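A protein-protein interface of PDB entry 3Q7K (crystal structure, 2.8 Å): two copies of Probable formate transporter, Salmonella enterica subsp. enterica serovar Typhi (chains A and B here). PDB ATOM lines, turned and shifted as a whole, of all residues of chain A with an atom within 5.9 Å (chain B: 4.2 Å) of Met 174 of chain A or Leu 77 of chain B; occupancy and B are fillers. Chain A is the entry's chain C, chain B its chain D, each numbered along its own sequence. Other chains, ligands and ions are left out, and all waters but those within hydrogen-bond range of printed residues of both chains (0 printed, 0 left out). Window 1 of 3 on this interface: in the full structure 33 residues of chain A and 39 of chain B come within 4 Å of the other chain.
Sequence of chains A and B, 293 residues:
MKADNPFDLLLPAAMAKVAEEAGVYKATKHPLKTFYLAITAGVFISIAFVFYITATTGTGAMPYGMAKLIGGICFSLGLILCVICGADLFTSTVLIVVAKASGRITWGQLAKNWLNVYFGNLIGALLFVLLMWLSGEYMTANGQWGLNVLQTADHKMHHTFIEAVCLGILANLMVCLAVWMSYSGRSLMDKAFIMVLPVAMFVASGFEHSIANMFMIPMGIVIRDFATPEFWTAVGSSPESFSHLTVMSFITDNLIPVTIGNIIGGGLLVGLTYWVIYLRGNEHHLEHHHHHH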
ATOM      1  N   ILE A 169      29.027  -1.265 -16.385  1.00  0.00           N
ATOM      2  CA  ILE A 169      29.277  -0.404 -15.235  1.00  0.00           C
ATOM      3  C   ILE A 169      28.036   0.408 -15.005  1.00  0.00           C
ATOM      4  O   ILE A 169      27.526   0.514 -13.875  1.00  0.00           O
ATOM      5  CB  ILE A 169      30.479   0.527 -15.489  1.00  0.00           C
ATOM      6  CG1 ILE A 169      31.787  -0.275 -15.402  1.00  0.00           C
ATOM      7  CG2 ILE A 169      30.487   1.685 -14.532  1.00  0.00           C
ATOM      8  CD1 ILE A 169      33.016   0.554 -15.789  1.00  0.00           C
ATOM      9  N   LEU A 170      27.531   0.967 -16.103  1.00  0.00           N
ATOM     10  CA  LEU A 170      26.330   1.774 -16.066  1.00  0.00           C
ATOM     11  C   LEU A 170      25.122   0.995 -15.498  1.00  0.00           C
ATOM     12  O   LEU A 170      24.387   1.529 -14.665  1.00  0.00           O
ATOM     13  CB  LEU A 170      26.052   2.339 -17.450  1.00  0.00           C
ATOM     14  CG  LEU A 170      26.964   3.437 -18.003  1.00  0.00           C
ATOM     15  CD1 LEU A 170      26.697   3.657 -19.472  1.00  0.00           C
ATOM     16  CD2 LEU A 170      26.738   4.721 -17.325  1.00  0.00           C
ATOM     17  N   ALA A 171      24.943  -0.265 -15.909  1.00  0.00           N
ATOM     18  CA  ALA A 171      23.771  -1.003 -15.501  1.00  0.00           C
ATOM     19  C   ALA A 171      23.822  -1.244 -14.008  1.00  0.00           C
ATOM     20  O   ALA A 171      22.897  -0.894 -13.279  1.00  0.00           O
ATOM     21  CB  ALA A 171      23.651  -2.281 -16.257  1.00  0.00           C
ATOM     22  N   ASN A 172      24.922  -1.802 -13.539  1.00  0.00           N
ATOM     23  CA  ASN A 172      24.985  -2.236 -12.145  1.00  0.00           C
ATOM     24  C   ASN A 172      25.048  -1.064 -11.142  1.00  0.00           C
ATOM     25  O   ASN A 172      24.657  -1.225  -9.979  1.00  0.00           O
ATOM     26  CB  ASN A 172      26.091  -3.270 -11.933  1.00  0.00           C
ATOM     27  CG  ASN A 172      25.812  -4.167 -10.753  1.00  0.00           C
ATOM     28  OD1 ASN A 172      24.649  -4.520 -10.487  1.00  0.00           O
ATOM     29  ND2 ASN A 172      26.871  -4.543 -10.018  1.00  0.00           N
ATOM     30  N   LEU A 173      25.518   0.105 -11.604  1.00  0.00           N
ATOM     31  CA  LEU A 173      25.453   1.360 -10.836  1.00  0.00           C
ATOM     32  C   LEU A 173      23.989   1.604 -10.538  1.00  0.00           C
ATOM     33  O   LEU A 173      23.599   1.824  -9.408  1.00  0.00           O
ATOM     34  CB  LEU A 173      26.003   2.530 -11.662  1.00  0.00           C
ATOM     35  CG  LEU A 173      26.705   3.761 -11.048  1.00  0.00           C
ATOM     36  CD1 LEU A 173      26.277   5.064 -11.730  1.00  0.00           C
ATOM     37  CD2 LEU A 173      26.492   3.907  -9.560  1.00  0.00           C
ATOM     38  N   MET A 174      23.159   1.501 -11.573  1.00  0.00           N
ATOM     39  CA  MET A 174      21.719   1.701 -11.422  1.00  0.00           C
ATOM     40  C   MET A 174      21.046   0.687 -10.494  1.00  0.00           C
ATOM     41  O   MET A 174      20.396   1.107  -9.555  1.00  0.00           O
ATOM     42  CB  MET A 174      21.039   1.850 -12.769  1.00  0.00           C
ATOM     43  CG  MET A 174      21.643   3.007 -13.607  1.00  0.00           C
ATOM     44  SD  MET A 174      21.756   4.716 -12.905  1.00  0.00           S
ATOM     45  CE  MET A 174      20.050   4.955 -12.374  1.00  0.00           C
ATOM     46  N   VAL A 175      21.231  -0.618 -10.720  1.00  0.00           N
ATOM     47  CA  VAL A 175      20.703  -1.653  -9.831  1.00  0.00           C
ATOM     48  C   VAL A 175      21.098  -1.399  -8.366  1.00  0.00           C
ATOM     49  O   VAL A 175      20.255  -1.436  -7.474  1.00  0.00           O
ATOM     50  CB  VAL A 175      21.179  -3.048 -10.241  1.00  0.00           C
ATOM     51  CG1 VAL A 175      20.792  -4.071  -9.193  1.00  0.00           C
ATOM     52  CG2 VAL A 175      20.623  -3.464 -11.591  1.00  0.00           C
ATOM     53  N   CYS A 176      22.369  -1.097  -8.124  1.00  0.00           N
ATOM     54  CA  CYS A 176      22.851  -0.755  -6.790  1.00  0.00           C
ATOM     55  C   CYS A 176      22.313   0.549  -6.199  1.00  0.00           C
ATOM     56  O   CYS A 176      22.011   0.635  -4.999  1.00  0.00           O
ATOM     57  CB  CYS A 176      24.367  -0.806  -6.750  1.00  0.00           C
ATOM     58  SG  CYS A 176      24.872  -2.561  -6.979  1.00  0.00           S
ATOM     59  N   LEU A 177      22.149   1.574  -7.009  1.00  0.00           N
ATOM     60  CA  LEU A 177      21.527   2.742  -6.436  1.00  0.00           C
ATOM     61  C   LEU A 177      20.070   2.402  -6.027  1.00  0.00           C
ATOM     62  O   LEU A 177      19.584   2.839  -4.953  1.00  0.00           O
ATOM     63  CB  LEU A 177      21.572   3.900  -7.403  1.00  0.00           C
ATOM     64  CG  LEU A 177      22.920   4.591  -7.531  1.00  0.00           C
ATOM     65  CD1 LEU A 177      22.897   5.493  -8.771  1.00  0.00           C
ATOM     66  CD2 LEU A 177      23.278   5.396  -6.271  1.00  0.00           C
ATOM     67  N   ALA A 178      19.395   1.601  -6.873  1.00  0.00           N
ATOM     68  CA  ALA A 178      18.031   1.177  -6.626  1.00  0.00           C
ATOM     69  C   ALA A 178      17.904   0.417  -5.281  1.00  0.00           C
ATOM     70  O   ALA A 178      17.011   0.685  -4.461  1.00  0.00           O
ATOM     71  CB  ALA A 178      17.571   0.329  -7.720  1.00  0.00           C
ATOM     72  N   VAL A 179      18.808  -0.518  -5.044  1.00  0.00           N
ATOM     73  CA  VAL A 179      18.706  -1.301  -3.849  1.00  0.00           C
ATOM     74  C   VAL A 179      19.080  -0.399  -2.651  1.00  0.00           C
ATOM     75  O   VAL A 179      18.453  -0.459  -1.585  1.00  0.00           O
ATOM     76  CB  VAL A 179      19.528  -2.613  -3.981  1.00  0.00           C
ATOM     77  CG1 VAL A 179      19.525  -3.420  -2.691  1.00  0.00           C
ATOM     78  CG2 VAL A 179      18.977  -3.458  -5.122  1.00  0.00           C
ATOM     79  N   MET A 181      18.674   2.828  -2.235  1.00  0.00           N
ATOM     80  CA  MET A 181      17.533   3.665  -1.926  1.00  0.00           C
ATOM     81  C   MET A 181      16.412   2.873  -1.243  1.00  0.00           C
ATOM     82  O   MET A 181      15.783   3.351  -0.309  1.00  0.00           O
ATOM     83  CB  MET A 181      17.039   4.323  -3.194  1.00  0.00           C
ATOM     84  CG  MET A 181      17.904   5.462  -3.679  1.00  0.00           C
ATOM     85  SD  MET A 181      17.010   6.608  -4.793  1.00  0.00           S
ATOM     86  CE  MET A 181      16.737   5.611  -6.264  1.00  0.00           C
ATOM     87  N   LEU A 197      12.085   4.058 -11.269  1.00  0.00           N
ATOM     88  CA  LEU A 197      12.806   5.027 -12.101  1.00  0.00           C
ATOM     89  C   LEU A 197      14.272   4.634 -12.352  1.00  0.00           C
ATOM     90  O   LEU A 197      14.706   4.626 -13.486  1.00  0.00           O
ATOM     91  CB  LEU A 197      12.685   6.441 -11.535  1.00  0.00           C
ATOM     92  CG  LEU A 197      11.735   7.518 -12.105  1.00  0.00           C
ATOM     93  CD1 LEU A 197      10.584   6.964 -12.899  1.00  0.00           C
ATOM     94  CD2 LEU A 197      11.188   8.473 -11.056  1.00  0.00           C
ATOM     95  N   PRO A 198      15.039   4.254 -11.309  1.00  0.00           N
ATOM     96  CA  PRO A 198      16.424   3.941 -11.679  1.00  0.00           C
ATOM     97  C   PRO A 198      16.567   2.606 -12.495  1.00  0.00           C
ATOM     98  O   PRO A 198      17.513   2.462 -13.279  1.00  0.00           O
ATOM     99  CB  PRO A 198      17.137   3.892 -10.299  1.00  0.00           C
ATOM    100  CG  PRO A 198      16.100   3.388  -9.397  1.00  0.00           C
ATOM    101  CD  PRO A 198      14.802   4.001  -9.872  1.00  0.00           C
ATOM    102  N   VAL A 199      15.665   1.647 -12.323  1.00  0.00           N
ATOM    103  CA  VAL A 199      15.764   0.411 -13.108  1.00  0.00           C
ATOM    104  C   VAL A 199      15.298   0.696 -14.547  1.00  0.00           C
ATOM    105  O   VAL A 199      15.950   0.268 -15.531  1.00  0.00           O
ATOM    106  CB  VAL A 199      14.937  -0.711 -12.486  1.00  0.00           C
ATOM    107  CG1 VAL A 199      14.851  -1.893 -13.419  1.00  0.00           C
ATOM    108  CG2 VAL A 199      15.561  -1.093 -11.173  1.00  0.00           C
ATOM    109  N   MET A 201      15.511   3.309 -16.100  1.00  0.00           N
ATOM    110  CA  MET A 201      16.561   4.094 -16.747  1.00  0.00           C
ATOM    111  C   MET A 201      17.614   3.156 -17.333  1.00  0.00           C
ATOM    112  O   MET A 201      17.995   3.258 -18.527  1.00  0.00           O
ATOM    113  CB  MET A 201      17.155   5.104 -15.792  1.00  0.00           C
ATOM    114  CG  MET A 201      18.165   6.054 -16.401  1.00  0.00           C
ATOM    115  SD  MET A 201      19.800   5.309 -16.259  1.00  0.00           S
ATOM    116  CE  MET A 201      20.815   6.582 -17.055  1.00  0.00           C
ATOM    117  N   PHE A 202      18.059   2.188 -16.539  1.00  0.00           N
ATOM    118  CA  PHE A 202      19.115   1.345 -17.081  1.00  0.00           C
ATOM    119  C   PHE A 202      18.620   0.487 -18.229  1.00  0.00           C
ATOM    120  O   PHE A 202      19.314   0.411 -19.235  1.00  0.00           O
ATOM    121  CB  PHE A 202      19.927   0.602 -16.018  1.00  0.00           C
ATOM    122  CG  PHE A 202      19.588  -0.869 -15.836  1.00  0.00           C
ATOM    123  CD1 PHE A 202      19.902  -1.806 -16.838  1.00  0.00           C
ATOM    124  CD2 PHE A 202      19.045  -1.319 -14.610  1.00  0.00           C
ATOM    125  CE1 PHE A 202      19.657  -3.141 -16.659  1.00  0.00           C
ATOM    126  CE2 PHE A 202      18.772  -2.682 -14.397  1.00  0.00           C
ATOM    127  CZ  PHE A 202      19.085  -3.602 -15.418  1.00  0.00           C
ATOM    128  N   PHE A 207      21.571  -0.448 -21.136  1.00  0.00           N
ATOM    129  CA  PHE A 207      22.762  -0.804 -20.338  1.00  0.00           C
ATOM    130  C   PHE A 207      22.732  -2.315 -20.070  1.00  0.00           C
ATOM    131  O   PHE A 207      21.668  -2.939 -20.158  1.00  0.00           O
ATOM    132  CB  PHE A 207      22.824  -0.012 -19.031  1.00  0.00           C
ATOM    133  CG  PHE A 207      22.895   1.469 -19.219  1.00  0.00           C
ATOM    134  CD1 PHE A 207      23.229   2.028 -20.464  1.00  0.00           C
ATOM    135  CD2 PHE A 207      22.647   2.320 -18.156  1.00  0.00           C
ATOM    136  CE1 PHE A 207      23.286   3.380 -20.638  1.00  0.00           C
ATOM    137  CE2 PHE A 207      22.724   3.696 -18.345  1.00  0.00           C
ATOM    138  CZ  PHE A 207      23.046   4.209 -19.591  1.00  0.00           C
ATOM    139  N   ILE B  47      22.865  11.381 -15.067  1.00  0.00           N
ATOM    140  CA  ILE B  47      21.915  10.251 -15.142  1.00  0.00           C
ATOM    141  C   ILE B  47      20.516  10.761 -15.568  1.00  0.00           C
ATOM    142  O   ILE B  47      19.964  10.330 -16.610  1.00  0.00           O
ATOM    143  CB  ILE B  47      21.859   9.383 -13.821  1.00  0.00           C
ATOM    144  CG1 ILE B  47      23.066   8.443 -13.761  1.00  0.00           C
ATOM    145  CG2 ILE B  47      20.589   8.492 -13.772  1.00  0.00           C
ATOM    146  CD1 ILE B  47      23.398   7.896 -12.371  1.00  0.00           C
ATOM    147  N   PHE B  51      18.714   9.686 -18.983  1.00  0.00           N
ATOM    148  CA  PHE B  51      17.325   9.221 -18.961  1.00  0.00           C
ATOM    149  C   PHE B  51      16.459   9.997 -19.937  1.00  0.00           C
ATOM    150  O   PHE B  51      15.786   9.395 -20.767  1.00  0.00           O
ATOM    151  CB  PHE B  51      16.714   9.289 -17.568  1.00  0.00           C
ATOM    152  CG  PHE B  51      15.635   8.263 -17.324  1.00  0.00           C
ATOM    153  CD1 PHE B  51      15.127   7.478 -18.369  1.00  0.00           C
ATOM    154  CD2 PHE B  51      15.134   8.059 -16.044  1.00  0.00           C
ATOM    155  CE1 PHE B  51      14.120   6.497 -18.128  1.00  0.00           C
ATOM    156  CE2 PHE B  51      14.130   7.084 -15.798  1.00  0.00           C
ATOM    157  CZ  PHE B  51      13.614   6.302 -16.839  1.00  0.00           C
ATOM    158  N   CYS B  74      11.018  11.520 -16.446  1.00  0.00           N
ATOM    159  CA  CYS B  74      12.221  10.674 -16.334  1.00  0.00           C
ATOM    160  C   CYS B  74      13.352  11.436 -15.621  1.00  0.00           C
ATOM    161  O   CYS B  74      14.042  10.879 -14.740  1.00  0.00           O
ATOM    162  CB  CYS B  74      12.702  10.157 -17.705  1.00  0.00           C
ATOM    163  SG  CYS B  74      11.514   9.047 -18.527  1.00  0.00           S
ATOM    164  N   PHE B  75      13.520  12.703 -15.990  1.00  0.00           N
ATOM    165  CA  PHE B  75      14.640  13.488 -15.498  1.00  0.00           C
ATOM    166  C   PHE B  75      14.680  13.492 -13.969  1.00  0.00           C
ATOM    167  O   PHE B  75      15.749  13.493 -13.351  1.00  0.00           O
ATOM    168  CB  PHE B  75      14.551  14.928 -16.024  1.00  0.00           C
ATOM    169  CG  PHE B  75      15.779  15.726 -15.793  1.00  0.00           C
ATOM    170  CD1 PHE B  75      16.830  15.715 -16.738  1.00  0.00           C
ATOM    171  CD2 PHE B  75      15.915  16.485 -14.618  1.00  0.00           C
ATOM    172  CE1 PHE B  75      17.993  16.450 -16.519  1.00  0.00           C
ATOM    173  CE2 PHE B  75      17.092  17.248 -14.385  1.00  0.00           C
ATOM    174  CZ  PHE B  75      18.120  17.225 -15.332  1.00  0.00           C
ATOM    175  N   SER B  76      13.496  13.485 -13.366  1.00  0.00           N
ATOM    176  CA  SER B  76      13.359  13.739 -11.931  1.00  0.00           C
ATOM    177  C   SER B  76      14.060  12.650 -11.120  1.00  0.00           C
ATOM    178  O   SER B  76      14.306  12.823  -9.929  1.00  0.00           O
ATOM    179  CB  SER B  76      11.889  13.880 -11.541  1.00  0.00           C
ATOM    180  OG  SER B  76      11.269  12.604 -11.545  1.00  0.00           O
ATOM    181  N   LEU B  77      14.401  11.541 -11.770  1.00  0.00           N
ATOM    182  CA  LEU B  77      15.313  10.564 -11.171  1.00  0.00           C
ATOM    183  C   LEU B  77      16.495  11.247 -10.545  1.00  0.00           C
ATOM    184  O   LEU B  77      16.867  10.908  -9.445  1.00  0.00           O
ATOM    185  CB  LEU B  77      15.931   9.633 -12.212  1.00  0.00           C
ATOM    186  CG  LEU B  77      16.181   8.160 -11.900  1.00  0.00           C
ATOM    187  CD1 LEU B  77      17.302   7.747 -12.811  1.00  0.00           C
ATOM    188  CD2 LEU B  77      16.427   7.812 -10.420  1.00  0.00           C
ATOM    189  N   GLY B  78      17.113  12.181 -11.257  1.00  0.00           N
ATOM    190  CA  GLY B  78      18.346  12.794 -10.779  1.00  0.00           C
ATOM    191  C   GLY B  78      18.163  13.398  -9.387  1.00  0.00           C
ATOM    192  O   GLY B  78      18.944  13.133  -8.443  1.00  0.00           O
ATOM    193  N   LEU B  79      17.110  14.194  -9.257  1.00  0.00           N
ATOM    194  CA  LEU B  79      16.955  14.986  -8.080  1.00  0.00           C
ATOM    195  C   LEU B  79      16.561  14.035  -6.974  1.00  0.00           C
ATOM    196  O   LEU B  79      16.995  14.197  -5.822  1.00  0.00           O
ATOM    197  CB  LEU B  79      15.898  16.039  -8.314  1.00  0.00           C
ATOM    198  CG  LEU B  79      16.117  17.507  -8.009  1.00  0.00           C
ATOM    199  CD1 LEU B  79      15.004  17.835  -7.041  1.00  0.00           C
ATOM    200  CD2 LEU B  79      17.400  17.833  -7.335  1.00  0.00           C
ATOM    201  N   ILE B  80      15.760  13.023  -7.331  1.00  0.00           N
ATOM    202  CA  ILE B  80      15.343  11.967  -6.395  1.00  0.00           C
ATOM    203  C   ILE B  80      16.601  11.290  -5.851  1.00  0.00           C
ATOM    204  O   ILE B  80      16.717  11.043  -4.668  1.00  0.00           O
ATOM    205  CB  ILE B  80      14.356  10.940  -7.061  1.00  0.00           C
ATOM    206  CG1 ILE B  80      13.016  11.593  -7.257  1.00  0.00           C
ATOM    207  CG2 ILE B  80      14.160   9.682  -6.210  1.00  0.00           C
ATOM    208  CD1 ILE B  80      12.035  10.743  -8.014  1.00  0.00           C
ATOM    209  N   LEU B  81      17.547  11.000  -6.729  1.00  0.00           N
ATOM    210  CA  LEU B  81      18.780  10.362  -6.346  1.00  0.00           C
ATOM    211  C   LEU B  81      19.580  11.281  -5.388  1.00  0.00           C
ATOM    212  O   LEU B  81      20.100  10.802  -4.393  1.00  0.00           O
ATOM    213  CB  LEU B  81      19.559  10.069  -7.619  1.00  0.00           C
ATOM    214  CG  LEU B  81      20.034   8.668  -8.015  1.00  0.00           C
ATOM    215  CD1 LEU B  81      19.285   7.572  -7.319  1.00  0.00           C
ATOM    216  CD2 LEU B  81      20.040   8.487  -9.586  1.00  0.00           C
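Among the printed residues, merely in contact across the chains: Met 174 of chain A with Ile 47 of chain B (3.6 Å), Met 174 of chain A with Leu 77 of chain B (3.9 Å), Met 181 of chain A with Leu 81 of chain B (3.4 Å), Leu 197 of chain A with Phe 51 of chain B (3.4 Å), Leu 197 of chain A with Leu 77 of chain B (3.9 Å), Leu 197 of chain A with Ile 80 of chain B (3.9 Å), Pro 198 of chain A with Leu 77 of chain B (3.9 Å), Met 201 of chain A with Ile 47 of chain B (3.8 Å), Met 201 of chain A with Phe 51 of chain B (3.5 Å) and Met 201 of chain A with Leu 77 of chain B (3.99 Å).
Printed residues of chain B that touch a printed residue of chain A: Ile 47, Phe 51, Leu 77, Ile 80 and Leu 81.
Of the printed residues of chain A, Leu 77 of chain B touches Met 174 (3.9 Å), Leu 197 (3.9 Å), Pro 198 (3.9 Å) and Met 201 (3.99 Å).
Printed residues of chain A within 4 Å of Leu 81 of chain B: Met 181 (3.4 Å).
Of the printed residues of chain B, Pro 198 of chain A touches Leu 77 (3.9 Å).
Of the printed residues of chain A, Phe 51 of chain B touches Leu 197 (3.4 Å) and Met 201 (3.5 Å).
Of the printed residues of chain B, Leu 197 of chain A touches Phe 51 (3.4 Å), Leu 77 (3.9 Å) and Ile 80 (3.9 Å).
Of the printed residues of chain A, Ile 80 of chain B touches Leu 197 (3.9 Å).
Phe 207 of chain A touches none of the printed residues of chain B.
Cys 176 of chain A touches none of the printed residues of chain B.
The nearest printed residue of chain A that does not touch Leu 77 of chain B is Met 181 of chain A (4.7 Å).
The nearest printed residue of chain B that does not touch Met 201 of chain A is Cys 74 of chain B (6.6 Å).
No position is printed for both chains.
Of the 10 pairs that touch across the chains among the printed residues, none has its exchanged pair printed and touching as well.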
